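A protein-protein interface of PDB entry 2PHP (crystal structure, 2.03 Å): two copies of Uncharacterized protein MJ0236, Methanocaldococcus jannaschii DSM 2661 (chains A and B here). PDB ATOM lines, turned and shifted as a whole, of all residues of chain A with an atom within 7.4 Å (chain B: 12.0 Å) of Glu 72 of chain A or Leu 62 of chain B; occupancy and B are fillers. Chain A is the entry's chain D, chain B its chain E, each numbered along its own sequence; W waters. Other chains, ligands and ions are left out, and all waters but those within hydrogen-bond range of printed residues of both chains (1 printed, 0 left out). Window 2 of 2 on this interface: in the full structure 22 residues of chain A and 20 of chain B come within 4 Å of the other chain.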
ATOM      1  N   ILE A  12      16.130   5.960  15.267  1.00  0.00           N
ATOM      2  CA  ILE A  12      15.351   7.045  15.840  1.00  0.00           C
ATOM      3  C   ILE A  12      14.174   6.509  16.655  1.00  0.00           C
ATOM      4  O   ILE A  12      13.933   6.971  17.769  1.00  0.00           O
ATOM      5  CB  ILE A  12      14.819   7.992  14.741  1.00  0.00           C
ATOM      6  CG1 ILE A  12      15.983   8.728  14.081  1.00  0.00           C
ATOM      7  CG2 ILE A  12      13.857   9.013  15.342  1.00  0.00           C
ATOM      8  CD1 ILE A  12      16.810   9.551  15.066  1.00  0.00           C
ATOM      9  N   LEU A  15      15.506   5.003  19.971  1.00  0.00           N
ATOM     10  CA  LEU A  15      15.910   6.002  20.953  1.00  0.00           C
ATOM     11  C   LEU A  15      14.685   6.690  21.523  1.00  0.00           C
ATOM     12  O   LEU A  15      14.601   6.939  22.735  1.00  0.00           O
ATOM     13  CB  LEU A  15      16.838   7.039  20.313  1.00  0.00           C
ATOM     14  CG  LEU A  15      18.296   6.596  20.187  1.00  0.00           C
ATOM     15  CD1 LEU A  15      19.054   7.527  19.258  1.00  0.00           C
ATOM     16  CD2 LEU A  15      18.918   6.576  21.585  1.00  0.00           C
ATOM     17  N   ILE A  37      21.924   9.268  26.012  1.00  0.00           N
ATOM     18  CA  ILE A  37      21.752   7.896  25.564  1.00  0.00           C
ATOM     19  C   ILE A  37      21.893   7.949  24.052  1.00  0.00           C
ATOM     20  O   ILE A  37      21.366   8.856  23.399  1.00  0.00           O
ATOM     21  CB  ILE A  37      20.375   7.325  25.992  1.00  0.00           C
ATOM     22  CG1 ILE A  37      20.272   5.854  25.567  1.00  0.00           C
ATOM     23  CG2 ILE A  37      19.238   8.180  25.420  1.00  0.00           C
ATOM     24  CD1 ILE A  37      19.119   5.107  26.213  1.00  0.00           C
ATOM     25  N   ALA A  38      22.642   6.999  23.501  1.00  0.00           N
ATOM     26  CA  ALA A  38      22.888   6.969  22.068  1.00  0.00           C
ATOM     27  C   ALA A  38      22.787   5.567  21.500  1.00  0.00           C
ATOM     28  O   ALA A  38      22.873   4.581  22.230  1.00  0.00           O
ATOM     29  CB  ALA A  38      24.269   7.544  21.774  1.00  0.00           C
ATOM     30  N   GLU A  39      22.603   5.501  20.185  1.00  0.00           N
ATOM     31  CA  GLU A  39      22.492   4.237  19.464  1.00  0.00           C
ATOM     32  C   GLU A  39      23.022   4.446  18.050  1.00  0.00           C
ATOM     33  O   GLU A  39      22.763   5.478  17.424  1.00  0.00           O
ATOM     34  CB  GLU A  39      21.033   3.759  19.416  1.00  0.00           C
ATOM     35  CG  GLU A  39      20.892   2.316  18.921  1.00  0.00           C
ATOM     36  CD  GLU A  39      19.452   1.836  18.843  1.00  0.00           C
ATOM     37  OE1 GLU A  39      18.791   1.734  19.900  1.00  0.00           O
ATOM     38  OE2 GLU A  39      18.983   1.553  17.714  1.00  0.00           O
ATOM     39  N   PHE A  47      31.151   9.107  14.407  1.00  0.00           N
ATOM     40  CA  PHE A  47      30.082   9.569  15.279  1.00  0.00           C
ATOM     41  C   PHE A  47      28.795   9.959  14.558  1.00  0.00           C
ATOM     42  O   PHE A  47      27.709   9.842  15.125  1.00  0.00           O
ATOM     43  CB  PHE A  47      30.586  10.722  16.167  1.00  0.00           C
ATOM     44  CG  PHE A  47      30.673  12.056  15.469  1.00  0.00           C
ATOM     45  CD1 PHE A  47      29.606  12.950  15.518  1.00  0.00           C
ATOM     46  CD2 PHE A  47      31.821  12.425  14.780  1.00  0.00           C
ATOM     47  CE1 PHE A  47      29.682  14.199  14.888  1.00  0.00           C
ATOM     48  CE2 PHE A  47      31.910  13.665  14.148  1.00  0.00           C
ATOM     49  CZ  PHE A  47      30.843  14.555  14.201  1.00  0.00           C
ATOM     50  N   LYS A  48      28.905  10.397  13.309  1.00  0.00           N
ATOM     51  CA  LYS A  48      27.720  10.792  12.560  1.00  0.00           C
ATOM     52  C   LYS A  48      26.796   9.606  12.266  1.00  0.00           C
ATOM     53  O   LYS A  48      25.672   9.793  11.792  1.00  0.00           O
ATOM     54  CB  LYS A  48      28.115  11.503  11.258  1.00  0.00           C
ATOM     55  CG  LYS A  48      28.776  12.864  11.487  1.00  0.00           C
ATOM     56  CD  LYS A  48      29.028  13.595  10.171  1.00  0.00           C
ATOM     57  CE  LYS A  48      29.748  14.923  10.385  1.00  0.00           C
ATOM     58  NZ  LYS A  48      28.970  15.856  11.246  1.00  0.00           N
ATOM     59  N   VAL A  50      25.878   7.777  14.614  1.00  0.00           N
ATOM     60  CA  VAL A  50      25.282   7.583  15.928  1.00  0.00           C
ATOM     61  C   VAL A  50      24.344   8.738  16.249  1.00  0.00           C
ATOM     62  O   VAL A  50      24.691   9.898  16.050  1.00  0.00           O
ATOM     63  CB  VAL A  50      26.376   7.491  17.015  1.00  0.00           C
ATOM     64  CG1 VAL A  50      25.752   7.438  18.396  1.00  0.00           C
ATOM     65  CG2 VAL A  50      27.236   6.259  16.767  1.00  0.00           C
ATOM     66  N   ALA A  51      23.150   8.411  16.734  1.00  0.00           N
ATOM     67  CA  ALA A  51      22.162   9.423  17.095  1.00  0.00           C
ATOM     68  C   ALA A  51      22.051   9.492  18.617  1.00  0.00           C
ATOM     69  O   ALA A  51      22.383   8.534  19.317  1.00  0.00           O
ATOM     70  CB  ALA A  51      20.806   9.081  16.487  1.00  0.00           C
ATOM     71  N   ALA A  52      21.585  10.629  19.125  1.00  0.00           N
ATOM     72  CA  ALA A  52      21.437  10.818  20.566  1.00  0.00           C
ATOM     73  C   ALA A  52      20.802  12.173  20.850  1.00  0.00           C
ATOM     74  O   ALA A  52      20.471  12.917  19.923  1.00  0.00           O
ATOM     75  CB  ALA A  52      22.799  10.730  21.249  1.00  0.00           C
ATOM     76  N   LEU A  53      20.631  12.499  22.130  1.00  0.00           N
ATOM     77  CA  LEU A  53      20.047  13.785  22.497  1.00  0.00           C
ATOM     78  C   LEU A  53      21.016  14.904  22.131  1.00  0.00           C
ATOM     79  O   LEU A  53      22.230  14.739  22.217  1.00  0.00           O
ATOM     80  CB  LEU A  53      19.751  13.832  24.006  1.00  0.00           C
ATOM     81  CG  LEU A  53      18.639  12.901  24.512  1.00  0.00           C
ATOM     82  CD1 LEU A  53      18.660  12.860  26.032  1.00  0.00           C
ATOM     83  CD2 LEU A  53      17.276  13.381  23.994  1.00  0.00           C
ATOM     84  N   THR A  54      20.478  16.037  21.697  1.00  0.00           N
ATOM     85  CA  THR A  54      21.309  17.184  21.354  1.00  0.00           C
ATOM     86  C   THR A  54      21.637  17.909  22.652  1.00  0.00           C
ATOM     87  O   THR A  54      22.596  18.677  22.731  1.00  0.00           O
ATOM     88  CB  THR A  54      20.575  18.140  20.406  1.00  0.00           C
ATOM     89  OG1 THR A  54      19.287  18.452  20.950  1.00  0.00           O
ATOM     90  CG2 THR A  54      20.413  17.495  19.022  1.00  0.00           C
ATOM     91  N   GLY A  55      20.820  17.654  23.669  1.00  0.00           N
ATOM     92  CA  GLY A  55      21.038  18.242  24.978  1.00  0.00           C
ATOM     93  C   GLY A  55      21.530  17.137  25.892  1.00  0.00           C
ATOM     94  O   GLY A  55      22.499  16.456  25.578  1.00  0.00           O
ATOM     95  N   GLY A  69      16.441  18.546  24.707  1.00  0.00           N
ATOM     96  CA  GLY A  69      16.810  18.403  23.308  1.00  0.00           C
ATOM     97  C   GLY A  69      16.052  17.405  22.446  1.00  0.00           C
ATOM     98  O   GLY A  69      15.057  16.809  22.856  1.00  0.00           O
ATOM     99  N   ASP A  70      16.545  17.252  21.223  1.00  0.00           N
ATOM    100  CA  ASP A  70      15.973  16.344  20.238  1.00  0.00           C
ATOM    101  C   ASP A  70      16.947  15.204  19.995  1.00  0.00           C
ATOM    102  O   ASP A  70      18.123  15.281  20.349  1.00  0.00           O
ATOM    103  CB  ASP A  70      15.771  17.045  18.891  1.00  0.00           C
ATOM    104  CG  ASP A  70      14.887  18.258  18.978  1.00  0.00           C
ATOM    105  OD1 ASP A  70      13.771  18.155  19.526  1.00  0.00           O
ATOM    106  OD2 ASP A  70      15.309  19.320  18.474  1.00  0.00           O
ATOM    107  N   ILE A  71      16.446  14.147  19.372  1.00  0.00           N
ATOM    108  CA  ILE A  71      17.285  13.021  19.029  1.00  0.00           C
ATOM    109  C   ILE A  71      17.733  13.268  17.594  1.00  0.00           C
ATOM    110  O   ILE A  71      16.910  13.444  16.691  1.00  0.00           O
ATOM    111  CB  ILE A  71      16.511  11.712  19.155  1.00  0.00           C
ATOM    112  CG1 ILE A  71      16.413  11.341  20.638  1.00  0.00           C
ATOM    113  CG2 ILE A  71      17.195  10.612  18.366  1.00  0.00           C
ATOM    114  CD1 ILE A  71      15.536  10.157  20.914  1.00  0.00           C
ATOM    115  N   GLU A  72      19.048  13.316  17.405  1.00  0.00           N
ATOM    116  CA  GLU A  72      19.644  13.557  16.099  1.00  0.00           C
ATOM    117  C   GLU A  72      20.929  12.774  15.946  1.00  0.00           C
ATOM    118  O   GLU A  72      21.570  12.403  16.936  1.00  0.00           O
ATOM    119  CB  GLU A  72      19.959  15.041  15.928  1.00  0.00           C
ATOM    120  CG  GLU A  72      18.746  15.883  15.661  1.00  0.00           C
ATOM    121  CD  GLU A  72      18.422  15.941  14.189  1.00  0.00           C
ATOM    122  OE1 GLU A  72      18.495  14.883  13.517  1.00  0.00           O
ATOM    123  OE2 GLU A  72      18.095  17.053  13.714  1.00  0.00           O
ATOM    124  N   PHE A  73      21.302  12.523  14.697  1.00  0.00           N
ATOM    125  CA  PHE A  73      22.529  11.808  14.416  1.00  0.00           C
ATOM    126  C   PHE A  73      23.695  12.771  14.615  1.00  0.00           C
ATOM    127  O   PHE A  73      23.551  13.978  14.428  1.00  0.00           O
ATOM    128  CB  PHE A  73      22.488  11.259  12.992  1.00  0.00           C
ATOM    129  CG  PHE A  73      21.809   9.924  12.891  1.00  0.00           C
ATOM    130  CD1 PHE A  73      22.517   8.753  13.140  1.00  0.00           C
ATOM    131  CD2 PHE A  73      20.445   9.837  12.605  1.00  0.00           C
ATOM    132  CE1 PHE A  73      21.880   7.513  13.112  1.00  0.00           C
ATOM    133  CE2 PHE A  73      19.796   8.595  12.574  1.00  0.00           C
ATOM    134  CZ  PHE A  73      20.515   7.435  12.828  1.00  0.00           C
ATOM    135  N   GLY A  74      24.839  12.236  15.020  1.00  0.00           N
ATOM    136  CA  GLY A  74      26.008  13.066  15.250  1.00  0.00           C
ATOM    137  C   GLY A  74      25.830  14.015  16.424  1.00  0.00           C
ATOM    138  O   GLY A  74      26.487  15.056  16.489  1.00  0.00           O
ATOM    139  N   ALA A  75      24.951  13.665  17.358  1.00  0.00           N
ATOM    140  CA  ALA A  75      24.715  14.519  18.517  1.00  0.00           C
ATOM    141  C   ALA A  75      25.604  14.182  19.715  1.00  0.00           C
ATOM    142  O   ALA A  75      25.610  14.917  20.701  1.00  0.00           O
ATOM    143  CB  ALA A  75      23.240  14.455  18.931  1.00  0.00           C
ATOM    144  N   SER A  76      26.362  13.092  19.642  1.00  0.00           N
ATOM    145  CA  SER A  76      27.220  12.726  20.769  1.00  0.00           C
ATOM    146  C   SER A  76      28.549  12.050  20.419  1.00  0.00           C
ATOM    147  O   SER A  76      28.674  10.822  20.487  1.00  0.00           O
ATOM    148  CB  SER A  76      26.440  11.835  21.744  1.00  0.00           C
ATOM    149  OG  SER A  76      27.207  11.516  22.893  1.00  0.00           O
ATOM    150  N   ASN B  26      26.321  34.505  21.767  1.00  0.00           N
ATOM    151  CA  ASN B  26      26.851  33.280  21.195  1.00  0.00           C
ATOM    152  C   ASN B  26      27.716  32.745  22.324  1.00  0.00           C
ATOM    153  O   ASN B  26      28.944  32.706  22.242  1.00  0.00           O
ATOM    154  CB  ASN B  26      27.688  33.574  19.955  1.00  0.00           C
ATOM    155  CG  ASN B  26      26.876  34.234  18.858  1.00  0.00           C
ATOM    156  OD1 ASN B  26      26.447  35.380  18.992  1.00  0.00           O
ATOM    157  ND2 ASN B  26      26.649  33.508  17.769  1.00  0.00           N
ATOM    158  N   PHE B  27      27.035  32.358  23.393  1.00  0.00           N
ATOM    159  CA  PHE B  27      27.648  31.846  24.604  1.00  0.00           C
ATOM    160  C   PHE B  27      28.124  30.406  24.438  1.00  0.00           C
ATOM    161  O   PHE B  27      27.324  29.502  24.231  1.00  0.00           O
ATOM    162  CB  PHE B  27      26.618  31.964  25.733  1.00  0.00           C
ATOM    163  CG  PHE B  27      27.078  31.426  27.058  1.00  0.00           C
ATOM    164  CD1 PHE B  27      28.277  31.850  27.624  1.00  0.00           C
ATOM    165  CD2 PHE B  27      26.285  30.521  27.762  1.00  0.00           C
ATOM    166  CE1 PHE B  27      28.683  31.377  28.874  1.00  0.00           C
ATOM    167  CE2 PHE B  27      26.683  30.045  29.011  1.00  0.00           C
ATOM    168  CZ  PHE B  27      27.883  30.474  29.567  1.00  0.00           C
ATOM    169  N   THR B  28      29.429  30.188  24.532  1.00  0.00           N
ATOM    170  CA  THR B  28      29.967  28.843  24.388  1.00  0.00           C
ATOM    171  C   THR B  28      30.809  28.448  25.585  1.00  0.00           C
ATOM    172  O   THR B  28      31.318  27.331  25.645  1.00  0.00           O
ATOM    173  CB  THR B  28      30.849  28.716  23.127  1.00  0.00           C
ATOM    174  OG1 THR B  28      32.038  29.506  23.290  1.00  0.00           O
ATOM    175  CG2 THR B  28      30.087  29.195  21.893  1.00  0.00           C
ATOM    176  N   ILE B  30      30.485  27.134  28.300  1.00  0.00           N
ATOM    177  CA  ILE B  30      29.717  26.256  29.161  1.00  0.00           C
ATOM    178  C   ILE B  30      30.524  25.038  29.574  1.00  0.00           C
ATOM    179  O   ILE B  30      31.062  24.325  28.732  1.00  0.00           O
ATOM    180  CB  ILE B  30      28.434  25.802  28.440  1.00  0.00           C
ATOM    181  CG1 ILE B  30      27.689  27.033  27.916  1.00  0.00           C
ATOM    182  CG2 ILE B  30      27.550  24.986  29.385  1.00  0.00           C
ATOM    183  CD1 ILE B  30      26.440  26.715  27.130  1.00  0.00           C
ATOM    184  N   ILE B  58      23.085  24.364  29.282  1.00  0.00           N
ATOM    185  CA  ILE B  58      23.936  23.344  28.678  1.00  0.00           C
ATOM    186  C   ILE B  58      24.095  23.564  27.182  1.00  0.00           C
ATOM    187  O   ILE B  58      23.293  24.253  26.555  1.00  0.00           O
ATOM    188  CB  ILE B  58      23.353  21.923  28.881  1.00  0.00           C
ATOM    189  CG1 ILE B  58      21.971  21.829  28.224  1.00  0.00           C
ATOM    190  CG2 ILE B  58      23.275  21.582  30.380  1.00  0.00           C
ATOM    191  CD1 ILE B  58      21.352  20.445  28.297  1.00  0.00           C
ATOM    192  N   LYS B  59      25.142  22.985  26.612  1.00  0.00           N
ATOM    193  CA  LYS B  59      25.383  23.128  25.183  1.00  0.00           C
ATOM    194  C   LYS B  59      24.383  22.345  24.337  1.00  0.00           C
ATOM    195  O   LYS B  59      23.853  21.314  24.755  1.00  0.00           O
ATOM    196  CB  LYS B  59      26.787  22.643  24.810  1.00  0.00           C
ATOM    197  CG  LYS B  59      27.899  23.614  25.113  1.00  0.00           C
ATOM    198  CD  LYS B  59      29.240  23.071  24.644  1.00  0.00           C
ATOM    199  CE  LYS B  59      30.356  24.047  24.994  1.00  0.00           C
ATOM    200  NZ  LYS B  59      31.685  23.603  24.495  1.00  0.00           N
ATOM    201  N   ASN B  60      24.114  22.877  23.154  1.00  0.00           N
ATOM    202  CA  ASN B  60      23.251  22.214  22.195  1.00  0.00           C
ATOM    203  C   ASN B  60      24.323  21.708  21.244  1.00  0.00           C
ATOM    204  O   ASN B  60      24.859  22.477  20.449  1.00  0.00           O
ATOM    205  CB  ASN B  60      22.352  23.209  21.470  1.00  0.00           C
ATOM    206  CG  ASN B  60      21.463  22.535  20.442  1.00  0.00           C
ATOM    207  OD1 ASN B  60      21.860  21.550  19.815  1.00  0.00           O
ATOM    208  ND2 ASN B  60      20.262  23.065  20.254  1.00  0.00           N
ATOM    209  N   LYS B  61      24.660  20.429  21.363  1.00  0.00           N
ATOM    210  CA  LYS B  61      25.705  19.820  20.549  1.00  0.00           C
ATOM    211  C   LYS B  61      25.572  20.042  19.047  1.00  0.00           C
ATOM    212  O   LYS B  61      26.515  19.801  18.296  1.00  0.00           O
ATOM    213  CB  LYS B  61      25.808  18.329  20.879  1.00  0.00           C
ATOM    214  CG  LYS B  61      26.523  18.089  22.205  1.00  0.00           C
ATOM    215  CD  LYS B  61      26.214  16.733  22.826  1.00  0.00           C
ATOM    216  CE  LYS B  61      24.769  16.671  23.292  1.00  0.00           C
ATOM    217  NZ  LYS B  61      24.532  15.513  24.181  1.00  0.00           N
ATOM    218  N   LEU B  62      24.414  20.513  18.608  1.00  0.00           N
ATOM    219  CA  LEU B  62      24.214  20.783  17.190  1.00  0.00           C
ATOM    220  C   LEU B  62      24.453  22.264  16.903  1.00  0.00           C
ATOM    221  O   LEU B  62      24.343  22.713  15.761  1.00  0.00           O
ATOM    222  CB  LEU B  62      22.793  20.390  16.772  1.00  0.00           C
ATOM    223  CG  LEU B  62      22.663  19.188  15.824  1.00  0.00           C
ATOM    224  CD1 LEU B  62      23.568  18.042  16.273  1.00  0.00           C
ATOM    225  CD2 LEU B  62      21.201  18.751  15.771  1.00  0.00           C
ATOM    226  N   GLY B  63      24.794  23.015  17.947  1.00  0.00           N
ATOM    227  CA  GLY B  63      25.029  24.440  17.798  1.00  0.00           C
ATOM    228  C   GLY B  63      24.167  25.255  18.747  1.00  0.00           C
ATOM    229  O   GLY B  63      22.947  25.095  18.784  1.00  0.00           O
ATOM    230  N   GLY B  64      24.804  26.130  19.518  1.00  0.00           N
ATOM    231  CA  GLY B  64      24.074  26.956  20.461  1.00  0.00           C
ATOM    232  C   GLY B  64      23.987  26.303  21.827  1.00  0.00           C
ATOM    233  O   GLY B  64      24.788  25.430  22.157  1.00  0.00           O
ATOM    234  N   PHE B  65      23.004  26.717  22.622  1.00  0.00           N
ATOM    235  CA  PHE B  65      22.827  26.165  23.961  1.00  0.00           C
ATOM    236  C   PHE B  65      21.362  26.170  24.389  1.00  0.00           C
ATOM    237  O   PHE B  65      20.521  26.786  23.737  1.00  0.00           O
ATOM    238  CB  PHE B  65      23.669  26.969  24.963  1.00  0.00           C
ATOM    239  CG  PHE B  65      23.391  28.450  24.945  1.00  0.00           C
ATOM    240  CD1 PHE B  65      22.515  29.024  25.861  1.00  0.00           C
ATOM    241  CD2 PHE B  65      23.994  29.270  23.990  1.00  0.00           C
ATOM    242  CE1 PHE B  65      22.240  30.394  25.831  1.00  0.00           C
ATOM    243  CE2 PHE B  65      23.727  30.644  23.947  1.00  0.00           C
ATOM    244  CZ  PHE B  65      22.846  31.205  24.871  1.00  0.00           C
ATOM    245  N   TYR B  66      21.075  25.474  25.487  1.00  0.00           N
ATOM    246  CA  TYR B  66      19.730  25.391  26.051  1.00  0.00           C
ATOM    247  C   TYR B  66      19.726  26.005  27.443  1.00  0.00           C
ATOM    248  O   TYR B  66      20.643  25.766  28.230  1.00  0.00           O
ATOM    249  CB  TYR B  66      19.284  23.936  26.216  1.00  0.00           C
ATOM    250  CG  TYR B  66      19.086  23.161  24.942  1.00  0.00           C
ATOM    251  CD1 TYR B  66      18.065  23.490  24.053  1.00  0.00           C
ATOM    252  CD2 TYR B  66      19.915  22.079  24.632  1.00  0.00           C
ATOM    253  CE1 TYR B  66      17.869  22.759  22.883  1.00  0.00           C
ATOM    254  CE2 TYR B  66      19.730  21.340  23.465  1.00  0.00           C
ATOM    255  CZ  TYR B  66      18.705  21.687  22.599  1.00  0.00           C
ATOM    256  OH  TYR B  66      18.499  20.958  21.450  1.00  0.00           O
ATOM    257  N   GLU B 185      38.988  29.949  21.175  1.00  0.00           N
ATOM    258  CA  GLU B 185      38.205  28.782  20.782  1.00  0.00           C
ATOM    259  C   GLU B 185      38.335  28.562  19.283  1.00  0.00           C
ATOM    260  O   GLU B 185      38.337  27.419  18.821  1.00  0.00           O
ATOM    261  CB  GLU B 185      36.731  28.975  21.145  1.00  0.00           C
ATOM    262  CG  GLU B 185      35.892  27.706  21.044  1.00  0.00           C
ATOM    263  CD  GLU B 185      34.433  27.924  21.425  1.00  0.00           C
ATOM    264  OE1 GLU B 185      33.689  26.925  21.522  1.00  0.00           O
ATOM    265  OE2 GLU B 185      34.027  29.089  21.622  1.00  0.00           O
HETATM  266  O   HOH W   1      26.948  13.176  25.104  1.00  0.00           O
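The side-chain amide nitrogen of Asn 60 of chain B sits at hydrogen-bond distance from the side-chain hydroxyl of Tyr 66 of chain B. N of Tyr 66 of chain B lies within hydrogen-bond range of O of Ile 58 of chain B (2.7 Å). The backbone NH of Thr 54 of chain A lies within hydrogen-bond range of the backbone carbonyl oxygen of Asp 70 of chain A, at 2.8 Å. N of Ala 52 of chain A lies within hydrogen-bond range of O of Glu 72 of chain A, at 2.8 Å. The side-chain amide oxygen of Asn 60 of chain B lies close to the backbone NH of Leu 62 of chain B, 3.0 Å away.
No position is printed for both chains.
Among the printed residues, pairs that only touch across the chains: Thr 54 of chain A with Lys 59 of chain B (3.6 Å), Thr 54 of chain A with Asn 60 of chain B (3.6 Å), Thr 54 of chain A with Leu 62 of chain B (3.6 Å), Gly 55 of chain A with Ile 58 of chain B (3.996 Å), Gly 55 of chain A with Tyr 66 of chain B (3.7 Å), Gly 69 of chain A with Tyr 66 of chain B (3.6 Å), Glu 72 of chain A with Leu 62 of chain B (3.8 Å) and Ala 75 of chain A with Lys 61 of chain B (2.9 Å).
The backbone carbonyl oxygen (O) of Leu 53 of chain A lies within hydrogen-bond range of the side-chain amino group (NZ) of Lys 61 of chain B, 3.1 Å away. O of Thr 54 of chain A lies close to N of Lys 61 of chain B (3.0 Å). The side-chain hydroxyl of Thr 54 of chain A is in hydrogen-bond range of the side-chain hydroxyl of Tyr 66 of chain B, at 2.7 Å. The backbone carbonyl oxygen (O) of Gly 55 of chain A is in hydrogen-bond range of the side-chain amino group (NZ) of Lys 61 of chain B.
Ile 12 of chain A touches none of the printed residues of chain B. Thr 54 of chain A touches just these residues of chain B: Lys 59 (3.6 Å), Asn 60 (3.6 Å), Lys 61 (3.0 Å), Leu 62 (3.6 Å) and Tyr 66 (2.7 Å). Printed residues of chain B within 4 Å of Gly 55 of chain A: Ile 58 (3.996 Å), Lys 61 (2.6 Å) and Tyr 66 (3.7 Å). Printed residues of chain B within 4 Å of Gly 69 of chain A: Tyr 66. No residue of chain B comes within 4 Å of Ile 71 of chain A. No residue of chain B comes within 4 Å of Phe 73 of chain A. Ala 75 of chain A touches just one residue of chain B: Lys 61. Of the printed residues of chain A, Asn 60 of chain B touches Thr 54 (3.6 Å). Leu 62 of chain B touches just these residues of chain A: Thr 54 and Glu 72. Glu 185 of chain B touches none of the printed residues of chain A. The nearest printed residue of chain B that does not touch Gly 69 of chain A is Ile 58 of chain B (6.4 Å).
Of the 21 printed residues of chain A, 6 touch a printed residue of chain B. Of the 14 printed residues of chain B, 6 touch a printed residue of chain A. Hydrophobic or aromatic side chains of chain B within 4 Å of the printed part of chain A: Ile 58, Leu 62 and Tyr 66. Among the printed residues, 12 pairs touch across the chains.
Water W1 bridges OG of Ser 76 of chain A (2.8 Å) and NZ of Lys 61 of chain B (3.5 Å).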
